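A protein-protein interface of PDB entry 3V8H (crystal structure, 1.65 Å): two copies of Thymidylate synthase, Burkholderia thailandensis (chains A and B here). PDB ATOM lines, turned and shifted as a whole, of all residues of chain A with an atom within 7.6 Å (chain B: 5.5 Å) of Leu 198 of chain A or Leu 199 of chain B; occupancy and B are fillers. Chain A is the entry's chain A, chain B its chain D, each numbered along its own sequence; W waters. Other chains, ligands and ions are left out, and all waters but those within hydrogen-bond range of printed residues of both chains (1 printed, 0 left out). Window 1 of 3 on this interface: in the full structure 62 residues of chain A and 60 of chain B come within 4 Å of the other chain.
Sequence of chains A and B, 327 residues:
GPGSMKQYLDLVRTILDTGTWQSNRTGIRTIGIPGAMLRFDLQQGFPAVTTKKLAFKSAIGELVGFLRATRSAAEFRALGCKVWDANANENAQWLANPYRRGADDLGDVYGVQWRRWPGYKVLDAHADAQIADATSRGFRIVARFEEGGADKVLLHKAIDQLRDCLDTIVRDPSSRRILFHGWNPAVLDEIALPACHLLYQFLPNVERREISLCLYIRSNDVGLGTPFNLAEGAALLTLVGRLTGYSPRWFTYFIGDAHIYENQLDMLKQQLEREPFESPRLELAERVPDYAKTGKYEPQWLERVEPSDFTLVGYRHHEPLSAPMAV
Among the printed residues, pairs that only touch across the chains: His 181 of chain A with His 181 of chain B, Trp 183 of chain A with Leu 179 of chain B, Leu 198 of chain A with Leu 179 of chain B, Leu 198 of chain A with Leu 199 of chain B, Leu 199 of chain A with Leu 198 of chain B, Leu 199 of chain A with Tyr 216 of chain B, Tyr 216 of chain A with Leu 199 of chain B, Tyr 216 of chain A with Cys 214 of chain B, Arg 218 of chain A with Leu 179 of chain B and Phe 254 of chain A with Tyr 216 of chain B.
Leu 198 of chain A touches just these residues of chain B: Leu 179 (3.8 Å) and Leu 199 (3.7 Å). Leu 199 of chain B touches two residues of chain A. Of the printed residues of chain B, Arg 218 of chain A touches Leu 179 (3.6 Å) and Gln 201 (3.0 Å). Of the printed residues of chain B, Tyr 216 of chain A touches Leu 199 (3.6 Å), Gln 201 (2.6 Å) and Cys 214 (3.5 Å). Printed residues of chain A within 4 Å of Tyr 216 of chain B: Leu 199 (3.8 Å) and Phe 254 (3.6 Å). The nearest residue of chain B that does not touch Leu 198 of chain A is His 181 of chain B (5.1 Å). The nearest residue of chain A that does not touch Leu 199 of chain B is Leu 199 of chain A (5.4 Å).
Water W1 lies within hydrogen-bond range of O of Leu 179 of chain B (2.9 Å) and NE1 of Trp 183 of chain A (2.9 Å).
Printed residues of chain A that touch a printed residue of chain B: His 181, Trp 183, Leu 198, Leu 199, Tyr 216, Arg 218 and Phe 254. Hydrophobic or aromatic side chains of chain A that line the printed part of chain B: His 181, Trp 183, Leu 198, Leu 199, Tyr 216 and Phe 254. Along chain A the printed residues that touch a printed residue of chain B span positions 181 to 254. Of the 12 printed residues of chain B, 7 touch a printed residue of chain A. Hydrophobic or aromatic side chains of chain B within 4 Å of the printed part of chain A: Leu 179, His 181, Leu 198, Leu 199 and Tyr 216. Among the printed residues, 13 pairs touch across the chains.
His 181 of chain B touches its own counterpart, His 181 of chain A. Leu 198 of chain A touches Leu 199 of chain B, and with the chains exchanged Leu 199 of chain A touches Leu 198 of chain B.
The side-chain amide nitrogen (NE2) of Gln 161 of chain A sits at hydrogen-bond distance from the backbone carbonyl oxygen (O) of His 181 of chain A (2.9 Å). The backbone NH (N) of Gln 201 of chain B lies within hydrogen-bond range of the backbone carbonyl oxygen (O) of Cys 214 of chain B, 2.8 Å away.
The backbone carbonyl oxygen (O) of Trp 183 of chain A sits at hydrogen-bond distance from a ring nitrogen (NE2) of His 181 of chain B (2.8 Å). The side-chain amide nitrogen of Gln 201 of chain B sits at hydrogen-bond distance from the backbone carbonyl oxygen of Arg 218 of chain A. The side-chain amide oxygen (OE1) of Gln 201 of chain B sits at hydrogen-bond distance from the side-chain hydroxyl (OH) of Tyr 216 of chain A, 2.6 Å away.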
ATOM      1  N   TYR A 110       1.632 -30.292  -9.298  1.00  0.00           N
ATOM      2  CA  TYR A 110       1.092 -28.963  -9.619  1.00  0.00           C
ATOM      3  C   TYR A 110       1.320 -27.918  -8.548  1.00  0.00           C
ATOM      4  O   TYR A 110       2.418 -27.393  -8.457  1.00  0.00           O
ATOM      5  CB  TYR A 110      -0.355 -29.141  -9.966  1.00  0.00           C
ATOM      6  CG  TYR A 110      -0.634 -29.730 -11.335  1.00  0.00           C
ATOM      7  CD1 TYR A 110      -0.298 -29.023 -12.492  1.00  0.00           C
ATOM      8  CD2 TYR A 110      -1.253 -30.947 -11.474  1.00  0.00           C
ATOM      9  CE1 TYR A 110      -0.569 -29.545 -13.752  1.00  0.00           C
ATOM     10  CE2 TYR A 110      -1.528 -31.472 -12.720  1.00  0.00           C
ATOM     11  CZ  TYR A 110      -1.238 -30.728 -13.861  1.00  0.00           C
ATOM     12  OH  TYR A 110      -1.540 -31.237 -15.113  1.00  0.00           O
ATOM     13  N   TRP A 114       4.185 -25.178  -7.569  1.00  0.00           N
ATOM     14  CA  TRP A 114       3.923 -23.732  -7.730  1.00  0.00           C
ATOM     15  C   TRP A 114       4.248 -22.969  -6.477  1.00  0.00           C
ATOM     16  O   TRP A 114       4.786 -21.847  -6.556  1.00  0.00           O
ATOM     17  CB  TRP A 114       2.483 -23.417  -8.056  1.00  0.00           C
ATOM     18  CG  TRP A 114       1.924 -24.068  -9.280  1.00  0.00           C
ATOM     19  CD1 TRP A 114       2.569 -24.874 -10.212  1.00  0.00           C
ATOM     20  CD2 TRP A 114       0.569 -23.960  -9.722  1.00  0.00           C
ATOM     21  NE1 TRP A 114       1.677 -25.258 -11.193  1.00  0.00           N
ATOM     22  CE2 TRP A 114       0.478 -24.729 -10.959  1.00  0.00           C
ATOM     23  CE3 TRP A 114      -0.561 -23.296  -9.238  1.00  0.00           C
ATOM     24  CZ2 TRP A 114      -0.708 -24.810 -11.671  1.00  0.00           C
ATOM     25  CZ3 TRP A 114      -1.736 -23.393  -9.964  1.00  0.00           C
ATOM     26  CH2 TRP A 114      -1.794 -24.135 -11.156  1.00  0.00           C
ATOM     27  N   GLN A 161       6.936 -19.882  -5.898  1.00  0.00           N
ATOM     28  CA  GLN A 161       7.055 -19.198  -7.176  1.00  0.00           C
ATOM     29  C   GLN A 161       5.901 -18.261  -7.428  1.00  0.00           C
ATOM     30  O   GLN A 161       6.098 -17.197  -7.962  1.00  0.00           O
ATOM     31  CB  GLN A 161       7.097 -20.172  -8.340  1.00  0.00           C
ATOM     32  CG  GLN A 161       8.213 -21.178  -8.345  1.00  0.00           C
ATOM     33  CD  GLN A 161       8.118 -22.076  -9.570  1.00  0.00           C
ATOM     34  OE1 GLN A 161       8.493 -21.665 -10.690  1.00  0.00           O
ATOM     35  NE2 GLN A 161       7.517 -23.245  -9.391  1.00  0.00           N
ATOM     36  N   PHE A 180       6.002 -18.911 -13.353  1.00  0.00           N
ATOM     37  CA  PHE A 180       6.229 -20.112 -12.532  1.00  0.00           C
ATOM     38  C   PHE A 180       5.885 -21.309 -13.354  1.00  0.00           C
ATOM     39  O   PHE A 180       5.203 -21.222 -14.359  1.00  0.00           O
ATOM     40  CB  PHE A 180       5.376 -20.091 -11.258  1.00  0.00           C
ATOM     41  CG  PHE A 180       3.879 -20.206 -11.484  1.00  0.00           C
ATOM     42  CD1 PHE A 180       3.292 -21.450 -11.520  1.00  0.00           C
ATOM     43  CD2 PHE A 180       3.043 -19.067 -11.643  1.00  0.00           C
ATOM     44  CE1 PHE A 180       1.919 -21.623 -11.700  1.00  0.00           C
ATOM     45  CE2 PHE A 180       1.696 -19.234 -11.779  1.00  0.00           C
ATOM     46  CZ  PHE A 180       1.119 -20.481 -11.879  1.00  0.00           C
ATOM     47  N   HIS A 181       6.410 -22.465 -12.945  1.00  0.00           N
ATOM     48  CA  HIS A 181       5.988 -23.678 -13.624  1.00  0.00           C
ATOM     49  C   HIS A 181       6.058 -24.870 -12.744  1.00  0.00           C
ATOM     50  O   HIS A 181       6.576 -24.795 -11.618  1.00  0.00           O
ATOM     51  CB  HIS A 181       6.857 -23.896 -14.889  1.00  0.00           C
ATOM     52  CG  HIS A 181       8.259 -24.269 -14.589  1.00  0.00           C
ATOM     53  ND1 HIS A 181       8.600 -25.517 -14.191  1.00  0.00           N
ATOM     54  CD2 HIS A 181       9.412 -23.519 -14.584  1.00  0.00           C
ATOM     55  CE1 HIS A 181       9.943 -25.570 -13.972  1.00  0.00           C
ATOM     56  NE2 HIS A 181      10.442 -24.356 -14.188  1.00  0.00           N
ATOM     57  N   GLY A 182       5.477 -25.994 -13.186  1.00  0.00           N
ATOM     58  CA  GLY A 182       5.387 -27.162 -12.331  1.00  0.00           C
ATOM     59  C   GLY A 182       6.122 -28.375 -12.820  1.00  0.00           C
ATOM     60  O   GLY A 182       5.745 -29.480 -12.497  1.00  0.00           O
ATOM     61  N   TRP A 183       7.143 -28.180 -13.675  1.00  0.00           N
ATOM     62  CA  TRP A 183       7.893 -29.301 -14.183  1.00  0.00           C
ATOM     63  C   TRP A 183       9.209 -29.382 -13.480  1.00  0.00           C
ATOM     64  O   TRP A 183      10.235 -28.771 -13.919  1.00  0.00           O
ATOM     65  CB  TRP A 183       8.137 -29.127 -15.669  1.00  0.00           C
ATOM     66  CG  TRP A 183       8.648 -30.389 -16.316  1.00  0.00           C
ATOM     67  CD1 TRP A 183       9.946 -30.731 -16.559  1.00  0.00           C
ATOM     68  CD2 TRP A 183       7.839 -31.450 -16.912  1.00  0.00           C
ATOM     69  NE1 TRP A 183      10.041 -31.946 -17.211  1.00  0.00           N
ATOM     70  CE2 TRP A 183       8.798 -32.474 -17.387  1.00  0.00           C
ATOM     71  CE3 TRP A 183       6.482 -31.739 -16.926  1.00  0.00           C
ATOM     72  CZ2 TRP A 183       8.374 -33.625 -18.022  1.00  0.00           C
ATOM     73  CZ3 TRP A 183       6.051 -32.884 -17.560  1.00  0.00           C
ATOM     74  CH2 TRP A 183       6.965 -33.838 -18.076  1.00  0.00           C
ATOM     75  N   ASN A 184       9.245 -30.183 -12.424  1.00  0.00           N
ATOM     76  CA  ASN A 184      10.447 -30.382 -11.625  1.00  0.00           C
ATOM     77  C   ASN A 184      11.062 -31.755 -11.948  1.00  0.00           C
ATOM     78  O   ASN A 184      10.506 -32.772 -11.594  1.00  0.00           O
ATOM     79  CB  ASN A 184      10.097 -30.229 -10.147  1.00  0.00           C
ATOM     80  CG  ASN A 184      11.315 -30.396  -9.225  1.00  0.00           C
ATOM     81  OD1 ASN A 184      12.383 -30.760  -9.699  1.00  0.00           O
ATOM     82  ND2 ASN A 184      11.143 -30.152  -7.926  1.00  0.00           N
ATOM     83  N   PRO A 194       2.518 -36.219 -14.340  1.00  0.00           N
ATOM     84  CA  PRO A 194       3.361 -35.046 -14.591  1.00  0.00           C
ATOM     85  C   PRO A 194       2.546 -33.887 -15.202  1.00  0.00           C
ATOM     86  O   PRO A 194       1.513 -34.135 -15.831  1.00  0.00           O
ATOM     87  CB  PRO A 194       4.396 -35.576 -15.565  1.00  0.00           C
ATOM     88  CG  PRO A 194       3.684 -36.617 -16.308  1.00  0.00           C
ATOM     89  CD  PRO A 194       2.652 -37.240 -15.381  1.00  0.00           C
ATOM     90  N   ALA A 195       2.977 -32.654 -14.972  1.00  0.00           N
ATOM     91  CA  ALA A 195       2.196 -31.451 -15.274  1.00  0.00           C
ATOM     92  C   ALA A 195       1.833 -31.458 -16.749  1.00  0.00           C
ATOM     93  O   ALA A 195       2.733 -31.697 -17.596  1.00  0.00           O
ATOM     94  CB  ALA A 195       2.970 -30.185 -14.932  1.00  0.00           C
ATOM     95  N   CYS A 196       0.544 -31.261 -17.013  1.00  0.00           N
ATOM     96  CA  CYS A 196      -0.003 -31.059 -18.365  1.00  0.00           C
ATOM     97  C   CYS A 196      -0.021 -29.571 -18.628  1.00  0.00           C
ATOM     98  O   CYS A 196       0.577 -29.103 -19.604  1.00  0.00           O
ATOM     99  CB  CYS A 196      -1.437 -31.598 -18.504  1.00  0.00           C
ATOM    100  SG  CYS A 196      -1.565 -33.377 -18.426  1.00  0.00           S
ATOM    101  N   HIS A 197      -0.668 -28.809 -17.765  1.00  0.00           N
ATOM    102  CA  HIS A 197      -0.545 -27.348 -17.821  1.00  0.00           C
ATOM    103  C   HIS A 197       0.712 -27.039 -17.044  1.00  0.00           C
ATOM    104  O   HIS A 197       0.831 -27.395 -15.861  1.00  0.00           O
ATOM    105  CB  HIS A 197      -1.786 -26.613 -17.343  1.00  0.00           C
ATOM    106  CG  HIS A 197      -2.349 -27.107 -16.038  1.00  0.00           C
ATOM    107  ND1 HIS A 197      -2.148 -26.450 -14.860  1.00  0.00           N
ATOM    108  CD2 HIS A 197      -3.181 -28.191 -15.755  1.00  0.00           C
ATOM    109  CE1 HIS A 197      -2.786 -27.111 -13.870  1.00  0.00           C
ATOM    110  NE2 HIS A 197      -3.420 -28.188 -14.414  1.00  0.00           N
ATOM    111  N   LEU A 198       1.709 -26.476 -17.724  1.00  0.00           N
ATOM    112  CA  LEU A 198       3.067 -26.506 -17.231  1.00  0.00           C
ATOM    113  C   LEU A 198       3.613 -25.174 -16.769  1.00  0.00           C
ATOM    114  O   LEU A 198       4.027 -25.068 -15.621  1.00  0.00           O
ATOM    115  CB  LEU A 198       3.975 -27.153 -18.310  1.00  0.00           C
ATOM    116  CG  LEU A 198       5.278 -27.760 -17.906  1.00  0.00           C
ATOM    117  CD1 LEU A 198       5.606 -28.756 -19.014  1.00  0.00           C
ATOM    118  CD2 LEU A 198       6.314 -26.620 -17.788  1.00  0.00           C
ATOM    119  N   LEU A 199       3.556 -24.141 -17.612  1.00  0.00           N
ATOM    120  CA  LEU A 199       4.234 -22.895 -17.315  1.00  0.00           C
ATOM    121  C   LEU A 199       3.260 -21.759 -17.467  1.00  0.00           C
ATOM    122  O   LEU A 199       2.543 -21.715 -18.438  1.00  0.00           O
ATOM    123  CB  LEU A 199       5.407 -22.698 -18.278  1.00  0.00           C
ATOM    124  CG  LEU A 199       6.354 -21.516 -18.087  1.00  0.00           C
ATOM    125  CD1 LEU A 199       7.790 -21.685 -18.551  1.00  0.00           C
ATOM    126  CD2 LEU A 199       5.768 -20.296 -18.808  1.00  0.00           C
ATOM    127  N   TYR A 200       3.292 -20.850 -16.504  1.00  0.00           N
ATOM    128  CA  TYR A 200       2.428 -19.686 -16.489  1.00  0.00           C
ATOM    129  C   TYR A 200       3.329 -18.444 -16.409  1.00  0.00           C
ATOM    130  O   TYR A 200       4.085 -18.291 -15.465  1.00  0.00           O
ATOM    131  CB  TYR A 200       1.523 -19.733 -15.244  1.00  0.00           C
ATOM    132  CG  TYR A 200       0.478 -20.823 -15.206  1.00  0.00           C
ATOM    133  CD1 TYR A 200       0.838 -22.174 -15.022  1.00  0.00           C
ATOM    134  CD2 TYR A 200      -0.878 -20.505 -15.273  1.00  0.00           C
ATOM    135  CE1 TYR A 200      -0.137 -23.165 -14.964  1.00  0.00           C
ATOM    136  CE2 TYR A 200      -1.855 -21.488 -15.176  1.00  0.00           C
ATOM    137  CZ  TYR A 200      -1.476 -22.811 -15.020  1.00  0.00           C
ATOM    138  OH  TYR A 200      -2.437 -23.829 -14.950  1.00  0.00           O
ATOM    139  N   LEU A 215       0.173 -19.280 -21.066  1.00  0.00           N
ATOM    140  CA  LEU A 215       0.135 -20.573 -20.396  1.00  0.00           C
ATOM    141  C   LEU A 215       0.579 -21.615 -21.397  1.00  0.00           C
ATOM    142  O   LEU A 215      -0.054 -21.721 -22.468  1.00  0.00           O
ATOM    143  CB  LEU A 215      -1.313 -20.857 -19.915  1.00  0.00           C
ATOM    144  CG  LEU A 215      -1.664 -22.244 -19.405  1.00  0.00           C
ATOM    145  CD1 LEU A 215      -0.689 -22.796 -18.371  1.00  0.00           C
ATOM    146  CD2 LEU A 215      -3.091 -22.229 -18.846  1.00  0.00           C
ATOM    147  N   TYR A 216       1.631 -22.371 -21.059  1.00  0.00           N
ATOM    148  CA  TYR A 216       2.163 -23.438 -21.927  1.00  0.00           C
ATOM    149  C   TYR A 216       1.645 -24.775 -21.415  1.00  0.00           C
ATOM    150  O   TYR A 216       1.841 -25.126 -20.254  1.00  0.00           O
ATOM    151  CB  TYR A 216       3.677 -23.462 -21.996  1.00  0.00           C
ATOM    152  CG  TYR A 216       4.188 -24.535 -22.941  1.00  0.00           C
ATOM    153  CD1 TYR A 216       4.429 -25.822 -22.497  1.00  0.00           C
ATOM    154  CD2 TYR A 216       4.395 -24.254 -24.299  1.00  0.00           C
ATOM    155  CE1 TYR A 216       4.844 -26.819 -23.390  1.00  0.00           C
ATOM    156  CE2 TYR A 216       4.853 -25.237 -25.172  1.00  0.00           C
ATOM    157  CZ  TYR A 216       5.071 -26.496 -24.724  1.00  0.00           C
ATOM    158  OH  TYR A 216       5.526 -27.463 -25.633  1.00  0.00           O
ATOM    159  N   ILE A 217       0.984 -25.479 -22.324  1.00  0.00           N
ATOM    160  CA  ILE A 217       0.399 -26.814 -22.093  1.00  0.00           C
ATOM    161  C   ILE A 217       1.177 -27.874 -22.840  1.00  0.00           C
ATOM    162  O   ILE A 217       1.260 -27.835 -24.052  1.00  0.00           O
ATOM    163  CB  ILE A 217      -1.061 -26.884 -22.644  1.00  0.00           C
ATOM    164  CG1 ILE A 217      -1.907 -25.704 -22.190  1.00  0.00           C
ATOM    165  CG2 ILE A 217      -1.674 -28.278 -22.375  1.00  0.00           C
ATOM    166  CD1 ILE A 217      -2.162 -25.682 -20.696  1.00  0.00           C
ATOM    167  N   ARG A 218       1.726 -28.862 -22.127  1.00  0.00           N
ATOM    168  CA  ARG A 218       2.501 -29.909 -22.752  1.00  0.00           C
ATOM    169  C   ARG A 218       1.617 -30.806 -23.641  1.00  0.00           C
ATOM    170  O   ARG A 218       2.026 -31.253 -24.719  1.00  0.00           O
ATOM    171  CB  ARG A 218       3.166 -30.727 -21.600  1.00  0.00           C
ATOM    172  CG  ARG A 218       3.561 -32.111 -21.940  1.00  0.00           C
ATOM    173  CD  ARG A 218       4.172 -32.867 -20.758  1.00  0.00           C
ATOM    174  NE  ARG A 218       3.217 -33.356 -19.754  1.00  0.00           N
ATOM    175  CZ  ARG A 218       2.345 -34.349 -19.928  1.00  0.00           C
ATOM    176  NH1 ARG A 218       2.299 -35.030 -21.069  1.00  0.00           N
ATOM    177  NH2 ARG A 218       1.529 -34.707 -18.938  1.00  0.00           N
ATOM    178  N   SER A 219       0.432 -31.130 -23.149  1.00  0.00           N
ATOM    179  CA  SER A 219      -0.427 -32.115 -23.764  1.00  0.00           C
ATOM    180  C   SER A 219      -1.849 -31.849 -23.319  1.00  0.00           C
ATOM    181  O   SER A 219      -2.084 -31.562 -22.144  1.00  0.00           O
ATOM    182  CB  SER A 219       0.018 -33.510 -23.323  1.00  0.00           C
ATOM    183  OG  SER A 219      -0.811 -34.519 -23.862  1.00  0.00           O
ATOM    184  N   PHE A 254      -0.992 -21.853 -25.145  1.00  0.00           N
ATOM    185  CA  PHE A 254      -0.095 -22.444 -26.126  1.00  0.00           C
ATOM    186  C   PHE A 254      -0.101 -23.944 -25.883  1.00  0.00           C
ATOM    187  O   PHE A 254       0.121 -24.337 -24.738  1.00  0.00           O
ATOM    188  CB  PHE A 254       1.354 -21.939 -25.892  1.00  0.00           C
ATOM    189  CG  PHE A 254       1.595 -20.481 -26.183  1.00  0.00           C
ATOM    190  CD1 PHE A 254       1.231 -19.926 -27.376  1.00  0.00           C
ATOM    191  CD2 PHE A 254       2.310 -19.707 -25.279  1.00  0.00           C
ATOM    192  CE1 PHE A 254       1.570 -18.630 -27.662  1.00  0.00           C
ATOM    193  CE2 PHE A 254       2.637 -18.396 -25.572  1.00  0.00           C
ATOM    194  CZ  PHE A 254       2.241 -17.873 -26.760  1.00  0.00           C
ATOM    195  N   LEU B 179      10.342 -33.586 -23.165  1.00  0.00           N
ATOM    196  CA  LEU B 179      10.639 -32.150 -23.047  1.00  0.00           C
ATOM    197  C   LEU B 179      11.741 -31.907 -22.058  1.00  0.00           C
ATOM    198  O   LEU B 179      12.022 -32.743 -21.182  1.00  0.00           O
ATOM    199  CB  LEU B 179       9.410 -31.313 -22.676  1.00  0.00           C
ATOM    200  CG  LEU B 179       8.886 -31.392 -21.230  1.00  0.00           C
ATOM    201  CD1 LEU B 179       9.540 -30.353 -20.292  1.00  0.00           C
ATOM    202  CD2 LEU B 179       7.373 -31.260 -21.202  1.00  0.00           C
ATOM    203  N   PHE B 180      12.418 -30.789 -22.246  1.00  0.00           N
ATOM    204  CA  PHE B 180      13.403 -30.304 -21.292  1.00  0.00           C
ATOM    205  C   PHE B 180      13.306 -28.807 -21.174  1.00  0.00           C
ATOM    206  O   PHE B 180      12.803 -28.154 -22.056  1.00  0.00           O
ATOM    207  CB  PHE B 180      14.810 -30.722 -21.679  1.00  0.00           C
ATOM    208  CG  PHE B 180      15.369 -30.019 -22.904  1.00  0.00           C
ATOM    209  CD1 PHE B 180      15.255 -30.589 -24.167  1.00  0.00           C
ATOM    210  CD2 PHE B 180      16.096 -28.839 -22.790  1.00  0.00           C
ATOM    211  CE1 PHE B 180      15.785 -29.956 -25.285  1.00  0.00           C
ATOM    212  CE2 PHE B 180      16.614 -28.194 -23.915  1.00  0.00           C
ATOM    213  CZ  PHE B 180      16.466 -28.755 -25.164  1.00  0.00           C
ATOM    214  N   HIS B 181      13.761 -28.275 -20.049  1.00  0.00           N
ATOM    215  CA  HIS B 181      13.868 -26.859 -19.904  1.00  0.00           C
ATOM    216  C   HIS B 181      15.009 -26.442 -19.023  1.00  0.00           C
ATOM    217  O   HIS B 181      15.670 -27.277 -18.330  1.00  0.00           O
ATOM    218  CB  HIS B 181      12.549 -26.291 -19.453  1.00  0.00           C
ATOM    219  CG  HIS B 181      12.225 -26.637 -18.034  1.00  0.00           C
ATOM    220  ND1 HIS B 181      12.842 -26.011 -16.992  1.00  0.00           N
ATOM    221  CD2 HIS B 181      11.326 -27.523 -17.491  1.00  0.00           C
ATOM    222  CE1 HIS B 181      12.400 -26.541 -15.835  1.00  0.00           C
ATOM    223  NE2 HIS B 181      11.467 -27.472 -16.127  1.00  0.00           N
ATOM    224  N   GLY B 182      15.245 -25.133 -19.084  1.00  0.00           N
ATOM    225  CA  GLY B 182      16.349 -24.507 -18.419  1.00  0.00           C
ATOM    226  C   GLY B 182      16.025 -23.640 -17.220  1.00  0.00           C
ATOM    227  O   GLY B 182      16.947 -22.918 -16.765  1.00  0.00           O
ATOM    228  N   HIS B 197      15.029 -18.461 -23.906  1.00  0.00           N
ATOM    229  CA  HIS B 197      14.484 -19.593 -24.670  1.00  0.00           C
ATOM    230  C   HIS B 197      14.522 -20.742 -23.709  1.00  0.00           C
ATOM    231  O   HIS B 197      15.595 -21.283 -23.379  1.00  0.00           O
ATOM    232  CB  HIS B 197      15.187 -19.871 -25.981  1.00  0.00           C
ATOM    233  CG  HIS B 197      16.650 -20.002 -25.890  1.00  0.00           C
ATOM    234  ND1 HIS B 197      17.246 -21.195 -25.679  1.00  0.00           N
ATOM    235  CD2 HIS B 197      17.655 -19.065 -26.014  1.00  0.00           C
ATOM    236  CE1 HIS B 197      18.573 -21.021 -25.668  1.00  0.00           C
ATOM    237  NE2 HIS B 197      18.832 -19.718 -25.884  1.00  0.00           N
ATOM    238  N   LEU B 198      13.334 -21.143 -23.273  1.00  0.00           N
ATOM    239  CA  LEU B 198      13.152 -21.752 -21.957  1.00  0.00           C
ATOM    240  C   LEU B 198      12.828 -23.234 -22.001  1.00  0.00           C
ATOM    241  O   LEU B 198      13.517 -24.045 -21.373  1.00  0.00           O
ATOM    242  CB  LEU B 198      12.068 -20.971 -21.220  1.00  0.00           C
ATOM    243  CG  LEU B 198      11.928 -21.176 -19.700  1.00  0.00           C
ATOM    244  CD1 LEU B 198      11.223 -19.978 -19.048  1.00  0.00           C
ATOM    245  CD2 LEU B 198      11.236 -22.493 -19.338  1.00  0.00           C
ATOM    246  N   LEU B 199      11.788 -23.599 -22.730  1.00  0.00           N
ATOM    247  CA  LEU B 199      11.267 -24.969 -22.774  1.00  0.00           C
ATOM    248  C   LEU B 199      11.241 -25.471 -24.201  1.00  0.00           C
ATOM    249  O   LEU B 199      10.789 -24.755 -25.102  1.00  0.00           O
ATOM    250  CB  LEU B 199       9.861 -25.045 -22.169  1.00  0.00           C
ATOM    251  CG  LEU B 199       9.266 -26.445 -22.064  1.00  0.00           C
ATOM    252  CD1 LEU B 199       8.374 -26.579 -20.804  1.00  0.00           C
ATOM    253  CD2 LEU B 199       8.461 -26.862 -23.301  1.00  0.00           C
ATOM    254  N   TYR B 200      11.725 -26.693 -24.381  1.00  0.00           N
ATOM    255  CA  TYR B 200      11.763 -27.386 -25.664  1.00  0.00           C
ATOM    256  C   TYR B 200      11.016 -28.712 -25.522  1.00  0.00           C
ATOM    257  O   TYR B 200      11.361 -29.537 -24.659  1.00  0.00           O
ATOM    258  CB  TYR B 200      13.212 -27.678 -26.038  1.00  0.00           C
ATOM    259  CG  TYR B 200      14.107 -26.480 -26.278  1.00  0.00           C
ATOM    260  CD1 TYR B 200      14.565 -25.717 -25.224  1.00  0.00           C
ATOM    261  CD2 TYR B 200      14.580 -26.207 -27.557  1.00  0.00           C
ATOM    262  CE1 TYR B 200      15.402 -24.613 -25.445  1.00  0.00           C
ATOM    263  CE2 TYR B 200      15.414 -25.113 -27.792  1.00  0.00           C
ATOM    264  CZ  TYR B 200      15.810 -24.322 -26.730  1.00  0.00           C
ATOM    265  OH  TYR B 200      16.685 -23.243 -26.989  1.00  0.00           O
ATOM    266  N   GLN B 201      10.036 -28.949 -26.386  1.00  0.00           N
ATOM    267  CA  GLN B 201       9.266 -30.173 -26.398  1.00  0.00           C
ATOM    268  C   GLN B 201       9.351 -30.804 -27.781  1.00  0.00           C
ATOM    269  O   GLN B 201       9.089 -30.148 -28.760  1.00  0.00           O
ATOM    270  CB  GLN B 201       7.789 -29.954 -26.021  1.00  0.00           C
ATOM    271  CG  GLN B 201       6.946 -31.228 -26.085  1.00  0.00           C
ATOM    272  CD  GLN B 201       5.569 -31.072 -25.481  1.00  0.00           C
ATOM    273  OE1 GLN B 201       5.174 -29.957 -25.125  1.00  0.00           O
ATOM    274  NE2 GLN B 201       4.776 -32.129 -25.483  1.00  0.00           N
ATOM    275  N   CYS B 214       8.287 -27.783 -30.176  1.00  0.00           N
ATOM    276  CA  CYS B 214       7.636 -26.573 -29.677  1.00  0.00           C
ATOM    277  C   CYS B 214       8.638 -25.945 -28.729  1.00  0.00           C
ATOM    278  O   CYS B 214       9.225 -26.686 -27.916  1.00  0.00           O
ATOM    279  CB  CYS B 214       6.318 -26.867 -28.948  1.00  0.00           C
ATOM    280  SG  CYS B 214       4.993 -27.433 -30.031  1.00  0.00           S
ATOM    281  N   LEU B 215       8.793 -24.629 -28.813  1.00  0.00           N
ATOM    282  CA  LEU B 215       9.780 -23.877 -28.045  1.00  0.00           C
ATOM    283  C   LEU B 215       9.059 -22.743 -27.413  1.00  0.00           C
ATOM    284  O   LEU B 215       8.433 -21.992 -28.130  1.00  0.00           O
ATOM    285  CB  LEU B 215      10.877 -23.336 -28.970  1.00  0.00           C
ATOM    286  CG  LEU B 215      11.976 -22.445 -28.404  1.00  0.00           C
ATOM    287  CD1 LEU B 215      12.629 -23.004 -27.159  1.00  0.00           C
ATOM    288  CD2 LEU B 215      13.035 -22.357 -29.508  1.00  0.00           C
ATOM    289  N   TYR B 216       9.176 -22.620 -26.101  1.00  0.00           N
ATOM    290  CA  TYR B 216       8.598 -21.467 -25.379  1.00  0.00           C
ATOM    291  C   TYR B 216       9.702 -20.492 -25.031  1.00  0.00           C
ATOM    292  O   TYR B 216      10.654 -20.859 -24.384  1.00  0.00           O
ATOM    293  CB  TYR B 216       7.902 -21.898 -24.056  1.00  0.00           C
ATOM    294  CG  TYR B 216       7.189 -20.733 -23.393  1.00  0.00           C
ATOM    295  CD1 TYR B 216       7.854 -19.904 -22.489  1.00  0.00           C
ATOM    296  CD2 TYR B 216       5.868 -20.431 -23.724  1.00  0.00           C
ATOM    297  CE1 TYR B 216       7.230 -18.803 -21.935  1.00  0.00           C
ATOM    298  CE2 TYR B 216       5.208 -19.326 -23.159  1.00  0.00           C
ATOM    299  CZ  TYR B 216       5.904 -18.532 -22.265  1.00  0.00           C
ATOM    300  OH  TYR B 216       5.240 -17.456 -21.710  1.00  0.00           O
HETATM  301  O   HOH W   1      12.596 -32.821 -18.339  1.00  0.00           O
